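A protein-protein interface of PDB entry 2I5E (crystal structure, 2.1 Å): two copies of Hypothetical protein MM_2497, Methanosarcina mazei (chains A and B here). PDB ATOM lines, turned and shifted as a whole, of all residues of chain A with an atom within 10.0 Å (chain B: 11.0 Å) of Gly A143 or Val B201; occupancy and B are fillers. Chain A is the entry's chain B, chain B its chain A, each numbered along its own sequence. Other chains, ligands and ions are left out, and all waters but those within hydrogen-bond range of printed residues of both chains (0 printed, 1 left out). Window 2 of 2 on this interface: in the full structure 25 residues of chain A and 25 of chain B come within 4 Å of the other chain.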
ATOM      1  N   LEU A  76      35.305 -14.052 -11.131  1.00  0.00           N
ATOM      2  CA  LEU A  76      35.387 -12.901 -10.293  1.00  0.00           C
ATOM      3  C   LEU A  76      36.330 -13.060  -9.104  1.00  0.00           C
ATOM      4  O   LEU A  76      37.278 -12.264  -8.913  1.00  0.00           O
ATOM      5  CB  LEU A  76      33.968 -12.542  -9.857  1.00  0.00           C
ATOM      6  CG  LEU A  76      33.776 -11.354  -8.928  1.00  0.00           C
ATOM      7  CD1 LEU A  76      34.255 -10.088  -9.655  1.00  0.00           C
ATOM      8  CD2 LEU A  76      32.293 -11.287  -8.565  1.00  0.00           C
ATOM      9  N   ASN A  77      36.030 -14.040  -8.258  1.00  0.00           N
ATOM     10  CA  ASN A  77      36.794 -14.274  -7.027  1.00  0.00           C
ATOM     11  C   ASN A  77      38.268 -14.566  -7.263  1.00  0.00           C
ATOM     12  O   ASN A  77      39.137 -13.964  -6.626  1.00  0.00           O
ATOM     13  CB  ASN A  77      36.101 -15.366  -6.205  1.00  0.00           C
ATOM     14  CG  ASN A  77      34.731 -14.886  -5.776  1.00  0.00           C
ATOM     15  OD1 ASN A  77      34.611 -13.712  -5.482  1.00  0.00           O
ATOM     16  ND2 ASN A  77      33.693 -15.711  -5.912  1.00  0.00           N
ATOM     17  N   GLY A 121      24.718  -5.022  -0.119  1.00  0.00           N
ATOM     18  CA  GLY A 121      23.727  -4.838  -1.114  1.00  0.00           C
ATOM     19  C   GLY A 121      22.447  -5.569  -0.798  1.00  0.00           C
ATOM     20  O   GLY A 121      22.267  -6.223   0.280  1.00  0.00           O
ATOM     21  N   LYS A 122      21.509  -5.451  -1.752  1.00  0.00           N
ATOM     22  CA  LYS A 122      20.256  -6.181  -1.657  1.00  0.00           C
ATOM     23  C   LYS A 122      20.512  -7.688  -1.586  1.00  0.00           C
ATOM     24  O   LYS A 122      21.415  -8.182  -2.217  1.00  0.00           O
ATOM     25  CB  LYS A 122      19.360  -5.875  -2.861  1.00  0.00           C
ATOM     26  CG  LYS A 122      17.951  -6.418  -2.740  1.00  0.00           C
ATOM     27  CD  LYS A 122      17.098  -6.224  -4.110  1.00  0.00           C
ATOM     28  CE  LYS A 122      17.870  -6.694  -5.437  1.00  0.00           C
ATOM     29  NZ  LYS A 122      19.066  -5.821  -6.147  1.00  0.00           N
ATOM     30  N   GLY A 123      19.676  -8.452  -0.866  1.00  0.00           N
ATOM     31  CA  GLY A 123      19.767  -9.933  -0.992  1.00  0.00           C
ATOM     32  C   GLY A 123      21.057 -10.523  -0.373  1.00  0.00           C
ATOM     33  O   GLY A 123      21.486 -11.634  -0.750  1.00  0.00           O
ATOM     34  N   GLY A 124      21.748  -9.779   0.513  1.00  0.00           N
ATOM     35  CA  GLY A 124      22.969 -10.386   1.086  1.00  0.00           C
ATOM     36  C   GLY A 124      24.187 -10.256   0.257  1.00  0.00           C
ATOM     37  O   GLY A 124      25.221 -10.953   0.552  1.00  0.00           O
ATOM     38  N   GLY A 125      24.149  -9.401  -0.813  1.00  0.00           N
ATOM     39  CA  GLY A 125      25.430  -9.110  -1.515  1.00  0.00           C
ATOM     40  C   GLY A 125      26.336  -8.080  -0.869  1.00  0.00           C
ATOM     41  O   GLY A 125      26.055  -7.564   0.189  1.00  0.00           O
ATOM     42  N   THR A 126      27.451  -7.773  -1.543  1.00  0.00           N
ATOM     43  CA  THR A 126      28.433  -6.788  -1.057  1.00  0.00           C
ATOM     44  C   THR A 126      28.615  -5.812  -2.185  1.00  0.00           C
ATOM     45  O   THR A 126      28.923  -6.229  -3.305  1.00  0.00           O
ATOM     46  CB  THR A 126      29.842  -7.482  -0.805  1.00  0.00           C
ATOM     47  OG1 THR A 126      29.670  -8.586   0.078  1.00  0.00           O
ATOM     48  CG2 THR A 126      30.807  -6.509  -0.205  1.00  0.00           C
ATOM     49  N   ASN A 127      28.284  -4.554  -1.945  1.00  0.00           N
ATOM     50  CA  ASN A 127      28.346  -3.531  -2.977  1.00  0.00           C
ATOM     51  C   ASN A 127      29.692  -2.841  -3.048  1.00  0.00           C
ATOM     52  O   ASN A 127      30.169  -2.415  -4.129  1.00  0.00           O
ATOM     53  CB  ASN A 127      27.185  -2.521  -2.749  1.00  0.00           C
ATOM     54  CG  ASN A 127      25.888  -3.030  -3.334  1.00  0.00           C
ATOM     55  OD1 ASN A 127      25.809  -4.175  -3.947  1.00  0.00           O
ATOM     56  ND2 ASN A 127      24.851  -2.266  -3.118  1.00  0.00           N
ATOM     57  N   LYS A 140      34.926 -13.344  -1.618  1.00  0.00           N
ATOM     58  CA  LYS A 140      34.141 -14.438  -2.109  1.00  0.00           C
ATOM     59  C   LYS A 140      32.779 -13.864  -2.403  1.00  0.00           C
ATOM     60  O   LYS A 140      31.812 -13.968  -1.604  1.00  0.00           O
ATOM     61  CB  LYS A 140      34.037 -15.614  -1.096  1.00  0.00           C
ATOM     62  CG  LYS A 140      33.492 -16.924  -1.722  1.00  0.00           C
ATOM     63  CD  LYS A 140      33.415 -18.064  -0.675  1.00  0.00           C
ATOM     64  CE  LYS A 140      32.663 -19.330  -1.189  1.00  0.00           C
ATOM     65  NZ  LYS A 140      31.276 -19.052  -1.752  1.00  0.00           N
ATOM     66  N   TYR A 141      32.729 -13.262  -3.572  1.00  0.00           N
ATOM     67  CA  TYR A 141      31.513 -12.708  -4.079  1.00  0.00           C
ATOM     68  C   TYR A 141      30.587 -13.839  -4.555  1.00  0.00           C
ATOM     69  O   TYR A 141      31.008 -15.004  -4.737  1.00  0.00           O
ATOM     70  CB  TYR A 141      31.845 -11.662  -5.185  1.00  0.00           C
ATOM     71  CG  TYR A 141      32.375 -10.372  -4.586  1.00  0.00           C
ATOM     72  CD1 TYR A 141      33.727 -10.238  -4.249  1.00  0.00           C
ATOM     73  CD2 TYR A 141      31.521  -9.312  -4.317  1.00  0.00           C
ATOM     74  CE1 TYR A 141      34.243  -9.016  -3.660  1.00  0.00           C
ATOM     75  CE2 TYR A 141      32.006  -8.091  -3.752  1.00  0.00           C
ATOM     76  CZ  TYR A 141      33.378  -7.956  -3.432  1.00  0.00           C
ATOM     77  OH  TYR A 141      33.893  -6.774  -2.917  1.00  0.00           O
ATOM     78  N   TYR A 142      29.345 -13.449  -4.752  1.00  0.00           N
ATOM     79  CA  TYR A 142      28.260 -14.316  -5.082  1.00  0.00           C
ATOM     80  C   TYR A 142      27.628 -14.873  -3.807  1.00  0.00           C
ATOM     81  O   TYR A 142      28.226 -14.833  -2.731  1.00  0.00           O
ATOM     82  CB  TYR A 142      28.711 -15.411  -6.075  1.00  0.00           C
ATOM     83  CG  TYR A 142      29.084 -14.818  -7.425  1.00  0.00           C
ATOM     84  CD1 TYR A 142      28.218 -13.939  -8.074  1.00  0.00           C
ATOM     85  CD2 TYR A 142      30.311 -15.081  -8.000  1.00  0.00           C
ATOM     86  CE1 TYR A 142      28.574 -13.363  -9.314  1.00  0.00           C
ATOM     87  CE2 TYR A 142      30.670 -14.534  -9.226  1.00  0.00           C
ATOM     88  CZ  TYR A 142      29.794 -13.664  -9.877  1.00  0.00           C
ATOM     89  OH  TYR A 142      30.139 -13.110 -11.105  1.00  0.00           O
ATOM     90  N   GLY A 143      26.413 -15.361  -3.933  1.00  0.00           N
ATOM     91  CA  GLY A 143      25.730 -15.935  -2.804  1.00  0.00           C
ATOM     92  C   GLY A 143      25.685 -14.978  -1.642  1.00  0.00           C
ATOM     93  O   GLY A 143      25.525 -13.762  -1.791  1.00  0.00           O
ATOM     94  N   SER A 144      25.849 -15.560  -0.470  1.00  0.00           N
ATOM     95  CA  SER A 144      25.777 -14.814   0.756  1.00  0.00           C
ATOM     96  C   SER A 144      27.066 -14.129   1.192  1.00  0.00           C
ATOM     97  O   SER A 144      27.582 -14.371   2.326  1.00  0.00           O
ATOM     98  CB  SER A 144      25.237 -15.709   1.821  1.00  0.00           C
ATOM     99  OG  SER A 144      24.938 -14.915   2.914  1.00  0.00           O
ATOM    100  N   SER A 145      27.509 -13.176   0.350  1.00  0.00           N
ATOM    101  CA  SER A 145      28.795 -12.578   0.466  1.00  0.00           C
ATOM    102  C   SER A 145      28.968 -11.572   1.512  1.00  0.00           C
ATOM    103  O   SER A 145      30.068 -11.400   1.976  1.00  0.00           O
ATOM    104  CB  SER A 145      29.267 -11.958  -0.876  1.00  0.00           C
ATOM    105  OG  SER A 145      28.429 -10.846  -1.201  1.00  0.00           O
ATOM    106  N   PHE A 146      27.933 -10.816   1.843  1.00  0.00           N
ATOM    107  CA  PHE A 146      28.055  -9.811   2.894  1.00  0.00           C
ATOM    108  C   PHE A 146      28.475 -10.537   4.172  1.00  0.00           C
ATOM    109  O   PHE A 146      29.474 -10.160   4.795  1.00  0.00           O
ATOM    110  CB  PHE A 146      26.719  -9.067   3.151  1.00  0.00           C
ATOM    111  CG  PHE A 146      26.749  -8.165   4.367  1.00  0.00           C
ATOM    112  CD1 PHE A 146      27.382  -6.892   4.315  1.00  0.00           C
ATOM    113  CD2 PHE A 146      26.143  -8.554   5.522  1.00  0.00           C
ATOM    114  CE1 PHE A 146      27.398  -6.022   5.416  1.00  0.00           C
ATOM    115  CE2 PHE A 146      26.160  -7.734   6.695  1.00  0.00           C
ATOM    116  CZ  PHE A 146      26.811  -6.434   6.638  1.00  0.00           C
ATOM    117  N   LEU A 147      27.694 -11.504   4.606  1.00  0.00           N
ATOM    118  CA  LEU A 147      28.041 -12.207   5.852  1.00  0.00           C
ATOM    119  C   LEU A 147      29.355 -12.989   5.671  1.00  0.00           C
ATOM    120  O   LEU A 147      30.209 -12.949   6.575  1.00  0.00           O
ATOM    121  CB  LEU A 147      26.974 -13.167   6.327  1.00  0.00           C
ATOM    122  CG  LEU A 147      25.607 -12.657   6.779  1.00  0.00           C
ATOM    123  CD1 LEU A 147      24.678 -13.877   6.947  1.00  0.00           C
ATOM    124  CD2 LEU A 147      25.656 -11.689   8.010  1.00  0.00           C
ATOM    125  N   THR A 148      29.548 -13.700   4.553  1.00  0.00           N
ATOM    126  CA  THR A 148      30.876 -14.346   4.370  1.00  0.00           C
ATOM    127  C   THR A 148      32.107 -13.398   4.382  1.00  0.00           C
ATOM    128  O   THR A 148      33.172 -13.781   4.890  1.00  0.00           O
ATOM    129  CB  THR A 148      30.986 -15.561   3.411  1.00  0.00           C
ATOM    130  OG1 THR A 148      29.829 -15.714   2.586  1.00  0.00           O
ATOM    131  CG2 THR A 148      31.014 -16.881   4.318  1.00  0.00           C
ATOM    132  N   HIS A 149      31.961 -12.158   3.901  1.00  0.00           N
ATOM    133  CA  HIS A 149      33.037 -11.179   4.076  1.00  0.00           C
ATOM    134  C   HIS A 149      33.271 -10.736   5.498  1.00  0.00           C
ATOM    135  O   HIS A 149      34.412 -10.366   5.845  1.00  0.00           O
ATOM    136  CB  HIS A 149      32.863  -9.933   3.182  1.00  0.00           C
ATOM    137  CG  HIS A 149      33.134 -10.201   1.743  1.00  0.00           C
ATOM    138  ND1 HIS A 149      32.270  -9.805   0.732  1.00  0.00           N
ATOM    139  CD2 HIS A 149      34.100 -10.945   1.149  1.00  0.00           C
ATOM    140  CE1 HIS A 149      32.743 -10.242  -0.427  1.00  0.00           C
ATOM    141  NE2 HIS A 149      33.848 -10.931  -0.208  1.00  0.00           N
ATOM    142  N   ASP A 171      22.000  -1.470  -5.340  1.00  0.00           N
ATOM    143  CA  ASP A 171      22.610  -1.978  -6.541  1.00  0.00           C
ATOM    144  C   ASP A 171      21.482  -2.174  -7.544  1.00  0.00           C
ATOM    145  O   ASP A 171      20.355  -2.483  -7.171  1.00  0.00           O
ATOM    146  CB  ASP A 171      23.375  -3.281  -6.267  1.00  0.00           C
ATOM    147  CG  ASP A 171      22.560  -4.383  -5.536  1.00  0.00           C
ATOM    148  OD1 ASP A 171      22.306  -4.292  -4.300  1.00  0.00           O
ATOM    149  OD2 ASP A 171      22.350  -5.457  -6.158  1.00  0.00           O
ATOM    150  N   VAL B 179      14.382 -12.058   3.768  1.00  0.00           N
ATOM    151  CA  VAL B 179      15.801 -12.245   3.476  1.00  0.00           C
ATOM    152  C   VAL B 179      16.637 -11.188   4.204  1.00  0.00           C
ATOM    153  O   VAL B 179      17.604 -11.572   4.875  1.00  0.00           O
ATOM    154  CB  VAL B 179      16.088 -12.231   1.972  1.00  0.00           C
ATOM    155  CG1 VAL B 179      17.563 -12.649   1.693  1.00  0.00           C
ATOM    156  CG2 VAL B 179      15.184 -13.304   1.321  1.00  0.00           C
ATOM    157  N   GLU B 180      16.271  -9.897   4.137  1.00  0.00           N
ATOM    158  CA  GLU B 180      17.088  -8.850   4.706  1.00  0.00           C
ATOM    159  C   GLU B 180      17.023  -8.984   6.211  1.00  0.00           C
ATOM    160  O   GLU B 180      17.942  -8.691   6.889  1.00  0.00           O
ATOM    161  CB  GLU B 180      16.581  -7.420   4.346  1.00  0.00           C
ATOM    162  CG  GLU B 180      16.460  -7.096   2.864  1.00  0.00           C
ATOM    163  CD  GLU B 180      17.830  -7.152   2.176  1.00  0.00           C
ATOM    164  OE1 GLU B 180      18.890  -7.027   2.821  1.00  0.00           O
ATOM    165  OE2 GLU B 180      17.887  -7.411   0.986  1.00  0.00           O
ATOM    166  N   ILE B 183      19.332 -11.828   7.161  1.00  0.00           N
ATOM    167  CA  ILE B 183      20.736 -11.433   7.088  1.00  0.00           C
ATOM    168  C   ILE B 183      21.157 -10.413   8.173  1.00  0.00           C
ATOM    169  O   ILE B 183      22.192 -10.598   8.761  1.00  0.00           O
ATOM    170  CB  ILE B 183      21.110 -10.853   5.721  1.00  0.00           C
ATOM    171  CG1 ILE B 183      20.806 -11.899   4.627  1.00  0.00           C
ATOM    172  CG2 ILE B 183      22.527 -10.178   5.800  1.00  0.00           C
ATOM    173  CD1 ILE B 183      21.852 -12.785   4.192  1.00  0.00           C
ATOM    174  N   HIS B 184      20.369  -9.335   8.399  1.00  0.00           N
ATOM    175  CA  HIS B 184      20.827  -8.183   9.149  1.00  0.00           C
ATOM    176  C   HIS B 184      20.213  -8.024  10.510  1.00  0.00           C
ATOM    177  O   HIS B 184      20.665  -7.172  11.286  1.00  0.00           O
ATOM    178  CB  HIS B 184      20.574  -6.853   8.363  1.00  0.00           C
ATOM    179  CG  HIS B 184      21.358  -6.761   7.080  1.00  0.00           C
ATOM    180  ND1 HIS B 184      20.794  -6.969   5.832  1.00  0.00           N
ATOM    181  CD2 HIS B 184      22.671  -6.601   6.861  1.00  0.00           C
ATOM    182  CE1 HIS B 184      21.733  -6.912   4.893  1.00  0.00           C
ATOM    183  NE2 HIS B 184      22.873  -6.628   5.495  1.00  0.00           N
ATOM    184  N   ARG B 198      15.001 -20.761   6.260  1.00  0.00           N
ATOM    185  CA  ARG B 198      16.416 -20.626   6.137  1.00  0.00           C
ATOM    186  C   ARG B 198      16.723 -19.891   4.862  1.00  0.00           C
ATOM    187  O   ARG B 198      15.906 -19.857   3.939  1.00  0.00           O
ATOM    188  CB  ARG B 198      17.052 -22.054   6.047  1.00  0.00           C
ATOM    189  CG  ARG B 198      16.079 -23.046   5.538  1.00  0.00           C
ATOM    190  CD  ARG B 198      16.565 -24.480   5.612  1.00  0.00           C
ATOM    191  NE  ARG B 198      17.407 -24.532   4.500  1.00  0.00           N
ATOM    192  CZ  ARG B 198      17.276 -25.276   3.410  1.00  0.00           C
ATOM    193  NH1 ARG B 198      16.332 -26.186   3.252  1.00  0.00           N
ATOM    194  NH2 ARG B 198      18.209 -25.085   2.486  1.00  0.00           N
ATOM    195  N   LEU B 199      17.934 -19.337   4.765  1.00  0.00           N
ATOM    196  CA  LEU B 199      18.494 -18.847   3.484  1.00  0.00           C
ATOM    197  C   LEU B 199      19.151 -19.958   2.627  1.00  0.00           C
ATOM    198  O   LEU B 199      19.856 -20.799   3.103  1.00  0.00           O
ATOM    199  CB  LEU B 199      19.518 -17.734   3.778  1.00  0.00           C
ATOM    200  CG  LEU B 199      18.863 -16.613   4.616  1.00  0.00           C
ATOM    201  CD1 LEU B 199      19.830 -15.532   5.103  1.00  0.00           C
ATOM    202  CD2 LEU B 199      17.647 -15.933   3.842  1.00  0.00           C
ATOM    203  N   GLU B 200      18.937 -19.945   1.345  1.00  0.00           N
ATOM    204  CA  GLU B 200      19.579 -20.941   0.508  1.00  0.00           C
ATOM    205  C   GLU B 200      20.174 -20.251  -0.708  1.00  0.00           C
ATOM    206  O   GLU B 200      19.541 -19.362  -1.254  1.00  0.00           O
ATOM    207  CB  GLU B 200      18.488 -21.910   0.032  1.00  0.00           C
ATOM    208  CG  GLU B 200      18.801 -22.721  -1.184  1.00  0.00           C
ATOM    209  CD  GLU B 200      18.006 -23.996  -1.176  1.00  0.00           C
ATOM    210  OE1 GLU B 200      16.968 -24.003  -1.857  1.00  0.00           O
ATOM    211  OE2 GLU B 200      18.387 -24.941  -0.436  1.00  0.00           O
ATOM    212  N   VAL B 201      21.360 -20.658  -1.142  1.00  0.00           N
ATOM    213  CA  VAL B 201      21.958 -20.065  -2.333  1.00  0.00           C
ATOM    214  C   VAL B 201      21.633 -20.836  -3.627  1.00  0.00           C
ATOM    215  O   VAL B 201      22.019 -21.985  -3.748  1.00  0.00           O
ATOM    216  CB  VAL B 201      23.460 -19.957  -2.149  1.00  0.00           C
ATOM    217  CG1 VAL B 201      24.135 -19.456  -3.451  1.00  0.00           C
ATOM    218  CG2 VAL B 201      23.741 -19.018  -1.015  1.00  0.00           C
ATOM    219  N   LYS B 202      20.954 -20.233  -4.592  1.00  0.00           N
ATOM    220  CA  LYS B 202      20.848 -20.909  -5.867  1.00  0.00           C
ATOM    221  C   LYS B 202      21.355 -20.241  -7.155  1.00  0.00           C
ATOM    222  O   LYS B 202      22.073 -20.873  -7.925  1.00  0.00           O
ATOM    223  CB  LYS B 202      19.503 -21.656  -6.084  1.00  0.00           C
ATOM    224  CG  LYS B 202      18.284 -20.772  -6.352  1.00  0.00           C
ATOM    225  CD  LYS B 202      17.051 -21.517  -6.988  1.00  0.00           C
ATOM    226  CE  LYS B 202      16.235 -22.383  -5.954  1.00  0.00           C
ATOM    227  NZ  LYS B 202      15.459 -21.581  -4.911  1.00  0.00           N
ATOM    228  N   LYS B 203      21.070 -19.006  -7.498  1.00  0.00           N
ATOM    229  CA  LYS B 203      21.708 -18.726  -8.834  1.00  0.00           C
ATOM    230  C   LYS B 203      22.902 -17.850  -8.591  1.00  0.00           C
ATOM    231  O   LYS B 203      23.000 -16.729  -9.117  1.00  0.00           O
ATOM    232  CB  LYS B 203      20.706 -18.159  -9.871  1.00  0.00           C
ATOM    233  CG  LYS B 203      19.651 -19.180 -10.355  1.00  0.00           C
ATOM    234  CD  LYS B 203      20.254 -20.325 -11.174  1.00  0.00           C
ATOM    235  CE  LYS B 203      19.197 -20.861 -12.135  1.00  0.00           C
ATOM    236  NZ  LYS B 203      19.704 -20.962 -13.552  1.00  0.00           N
ATOM    237  N   GLY B 204      23.754 -18.319  -7.667  1.00  0.00           N
ATOM    238  CA  GLY B 204      24.644 -17.404  -7.032  1.00  0.00           C
ATOM    239  C   GLY B 204      23.807 -16.343  -6.325  1.00  0.00           C
ATOM    240  O   GLY B 204      24.313 -15.249  -6.026  1.00  0.00           O
ATOM    241  N   ARG B 205      22.547 -16.663  -6.006  1.00  0.00           N
ATOM    242  CA  ARG B 205      21.781 -15.733  -5.151  1.00  0.00           C
ATOM    243  C   ARG B 205      21.093 -16.351  -3.920  1.00  0.00           C
ATOM    244  O   ARG B 205      20.839 -17.528  -3.909  1.00  0.00           O
ATOM    245  CB  ARG B 205      20.938 -14.706  -5.975  1.00  0.00           C
ATOM    246  CG  ARG B 205      20.108 -15.270  -7.071  1.00  0.00           C
ATOM    247  CD  ARG B 205      20.091 -14.345  -8.374  1.00  0.00           C
ATOM    248  NE  ARG B 205      20.185 -12.889  -8.145  1.00  0.00           N
ATOM    249  CZ  ARG B 205      20.876 -11.995  -8.909  1.00  0.00           C
ATOM    250  NH1 ARG B 205      21.620 -12.328  -9.989  1.00  0.00           N
ATOM    251  NH2 ARG B 205      20.852 -10.721  -8.573  1.00  0.00           N
ATOM    252  N   VAL B 206      20.837 -15.544  -2.886  1.00  0.00           N
ATOM    253  CA  VAL B 206      20.184 -15.932  -1.622  1.00  0.00           C
ATOM    254  C   VAL B 206      18.659 -15.964  -1.787  1.00  0.00           C
ATOM    255  O   VAL B 206      18.069 -15.027  -2.343  1.00  0.00           O
ATOM    256  CB  VAL B 206      20.504 -14.964  -0.486  1.00  0.00           C
ATOM    257  CG1 VAL B 206      19.989 -15.508   0.879  1.00  0.00           C
ATOM    258  CG2 VAL B 206      21.946 -14.727  -0.354  1.00  0.00           C
ATOM    259  N   GLY B 207      18.007 -17.009  -1.288  1.00  0.00           N
ATOM    260  CA  GLY B 207      16.547 -17.125  -1.376  1.00  0.00           C
ATOM    261  C   GLY B 207      16.059 -17.622  -0.057  1.00  0.00           C
ATOM    262  O   GLY B 207      16.799 -18.323   0.640  1.00  0.00           O
ATOM    263  N   LEU B 208      14.816 -17.323   0.255  1.00  0.00           N
ATOM    264  CA  LEU B 208      14.134 -17.809   1.431  1.00  0.00           C
ATOM    265  C   LEU B 208      13.413 -19.133   1.180  1.00  0.00           C
ATOM    266  O   LEU B 208      12.616 -19.236   0.290  1.00  0.00           O
ATOM    267  CB  LEU B 208      13.126 -16.765   1.833  1.00  0.00           C
ATOM    268  CG  LEU B 208      12.361 -16.914   3.106  1.00  0.00           C
ATOM    269  CD1 LEU B 208      13.121 -16.272   4.134  1.00  0.00           C
ATOM    270  CD2 LEU B 208      11.077 -16.265   2.952  1.00  0.00           C
ATOM    271  N   VAL B 209      13.683 -20.139   1.974  1.00  0.00           N
ATOM    272  CA  VAL B 209      13.077 -21.428   1.746  1.00  0.00           C
ATOM    273  C   VAL B 209      12.626 -21.882   3.092  1.00  0.00           C
ATOM    274  O   VAL B 209      13.228 -21.482   4.067  1.00  0.00           O
ATOM    275  CB  VAL B 209      13.986 -22.426   0.991  1.00  0.00           C
ATOM    276  CG1 VAL B 209      14.152 -21.869  -0.432  1.00  0.00           C
ATOM    277  CG2 VAL B 209      15.360 -22.590   1.635  1.00  0.00           C
ATOM    278  N   PRO B 210      11.474 -22.586   3.153  1.00  0.00           N
ATOM    279  CA  PRO B 210      10.897 -23.049   4.464  1.00  0.00           C
ATOM    280  C   PRO B 210      11.738 -24.194   5.009  1.00  0.00           C
ATOM    281  O   PRO B 210      12.450 -24.832   4.241  1.00  0.00           O
ATOM    282  CB  PRO B 210       9.502 -23.573   4.081  1.00  0.00           C
ATOM    283  CG  PRO B 210       9.277 -23.093   2.581  1.00  0.00           C
ATOM    284  CD  PRO B 210      10.642 -23.002   1.987  1.00  0.00           C
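OG1 of Thr A126 is in hydrogen-bond range of N of Phe A146, at 3.3 Å.
O of Glu B180 lies within hydrogen-bond range of ND1 of His B184 (3.5 Å).
The side-chain carboxylate (OD2) of Asp A171 lies within salt-bridge range of the side-chain amino group (NZ) of Lys A122, at 3.3 Å.
O of Ser A144 lies within hydrogen-bond range of OG1 of Thr A148.
The backbone carbonyl oxygen (O) of Gly A124 sits at hydrogen-bond distance from the backbone NH (N) of Phe A146.
The backbone NH (N) of Gly A143 sits at hydrogen-bond distance from the backbone carbonyl oxygen (O) of Gly B204, 3.0 Å away.
OE2 of Glu B180 is in hydrogen-bond range of N of Gly A123 (2.8 Å).
No position is printed for both chains.
Gly A143 touches just these residues of chain B: Val B201 (3.9 Å), Gly B204 (3.0 Å) and Val B206 (3.96 Å).
Val B201 touches just one residue of chain A: Gly A143.
No residue of chain B comes within 4 Å of Gly A124.
No residue of chain B comes within 4 Å of Gly A125.
No residue of chain B comes within 4 Å of Ser A145.
Printed residues of chain A within 4 Å of Val B206: Gly A123, Gly A143 and Ser A144.
Of the printed residues of chain A, His B184 touches Phe A146.
Leu B199 touches none of the printed residues of chain A.
Thr A126 touches none of the printed residues of chain B.
The nearest residue of chain B that does not touch Gly A143 is Arg B205 (4.6 Å).
The nearest residue of chain A that does not touch Val B201 is Ser A144 (4.1 Å).
The nearest printed residue of chain B that does not touch Ser A144 is Val B201 (4.1 Å).
Among the printed residues, merely in contact across the chains: Lys A122 with Glu B180 (3.7 Å), Gly A123 with Val B206 (3.2 Å), Gly A143 with Val B201 (3.9 Å), Gly A143 with Val B206 (3.96 Å), Ser A144 with Ile B183 (3.96 Å), Ser A144 with Val B206 (3.99 Å), Phe A146 with Ile B183 (3.97 Å), Phe A146 with His B184 (3.7 Å) and Leu A147 with Ile B183 (3.7 Å).
Hydrophobic or aromatic side chains of chain B within 4 Å of the printed part of chain A: Ile B183, His B184, Val B201 and Val B206.
Of the 20 printed residues of chain A, 6 touch a printed residue of chain B.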
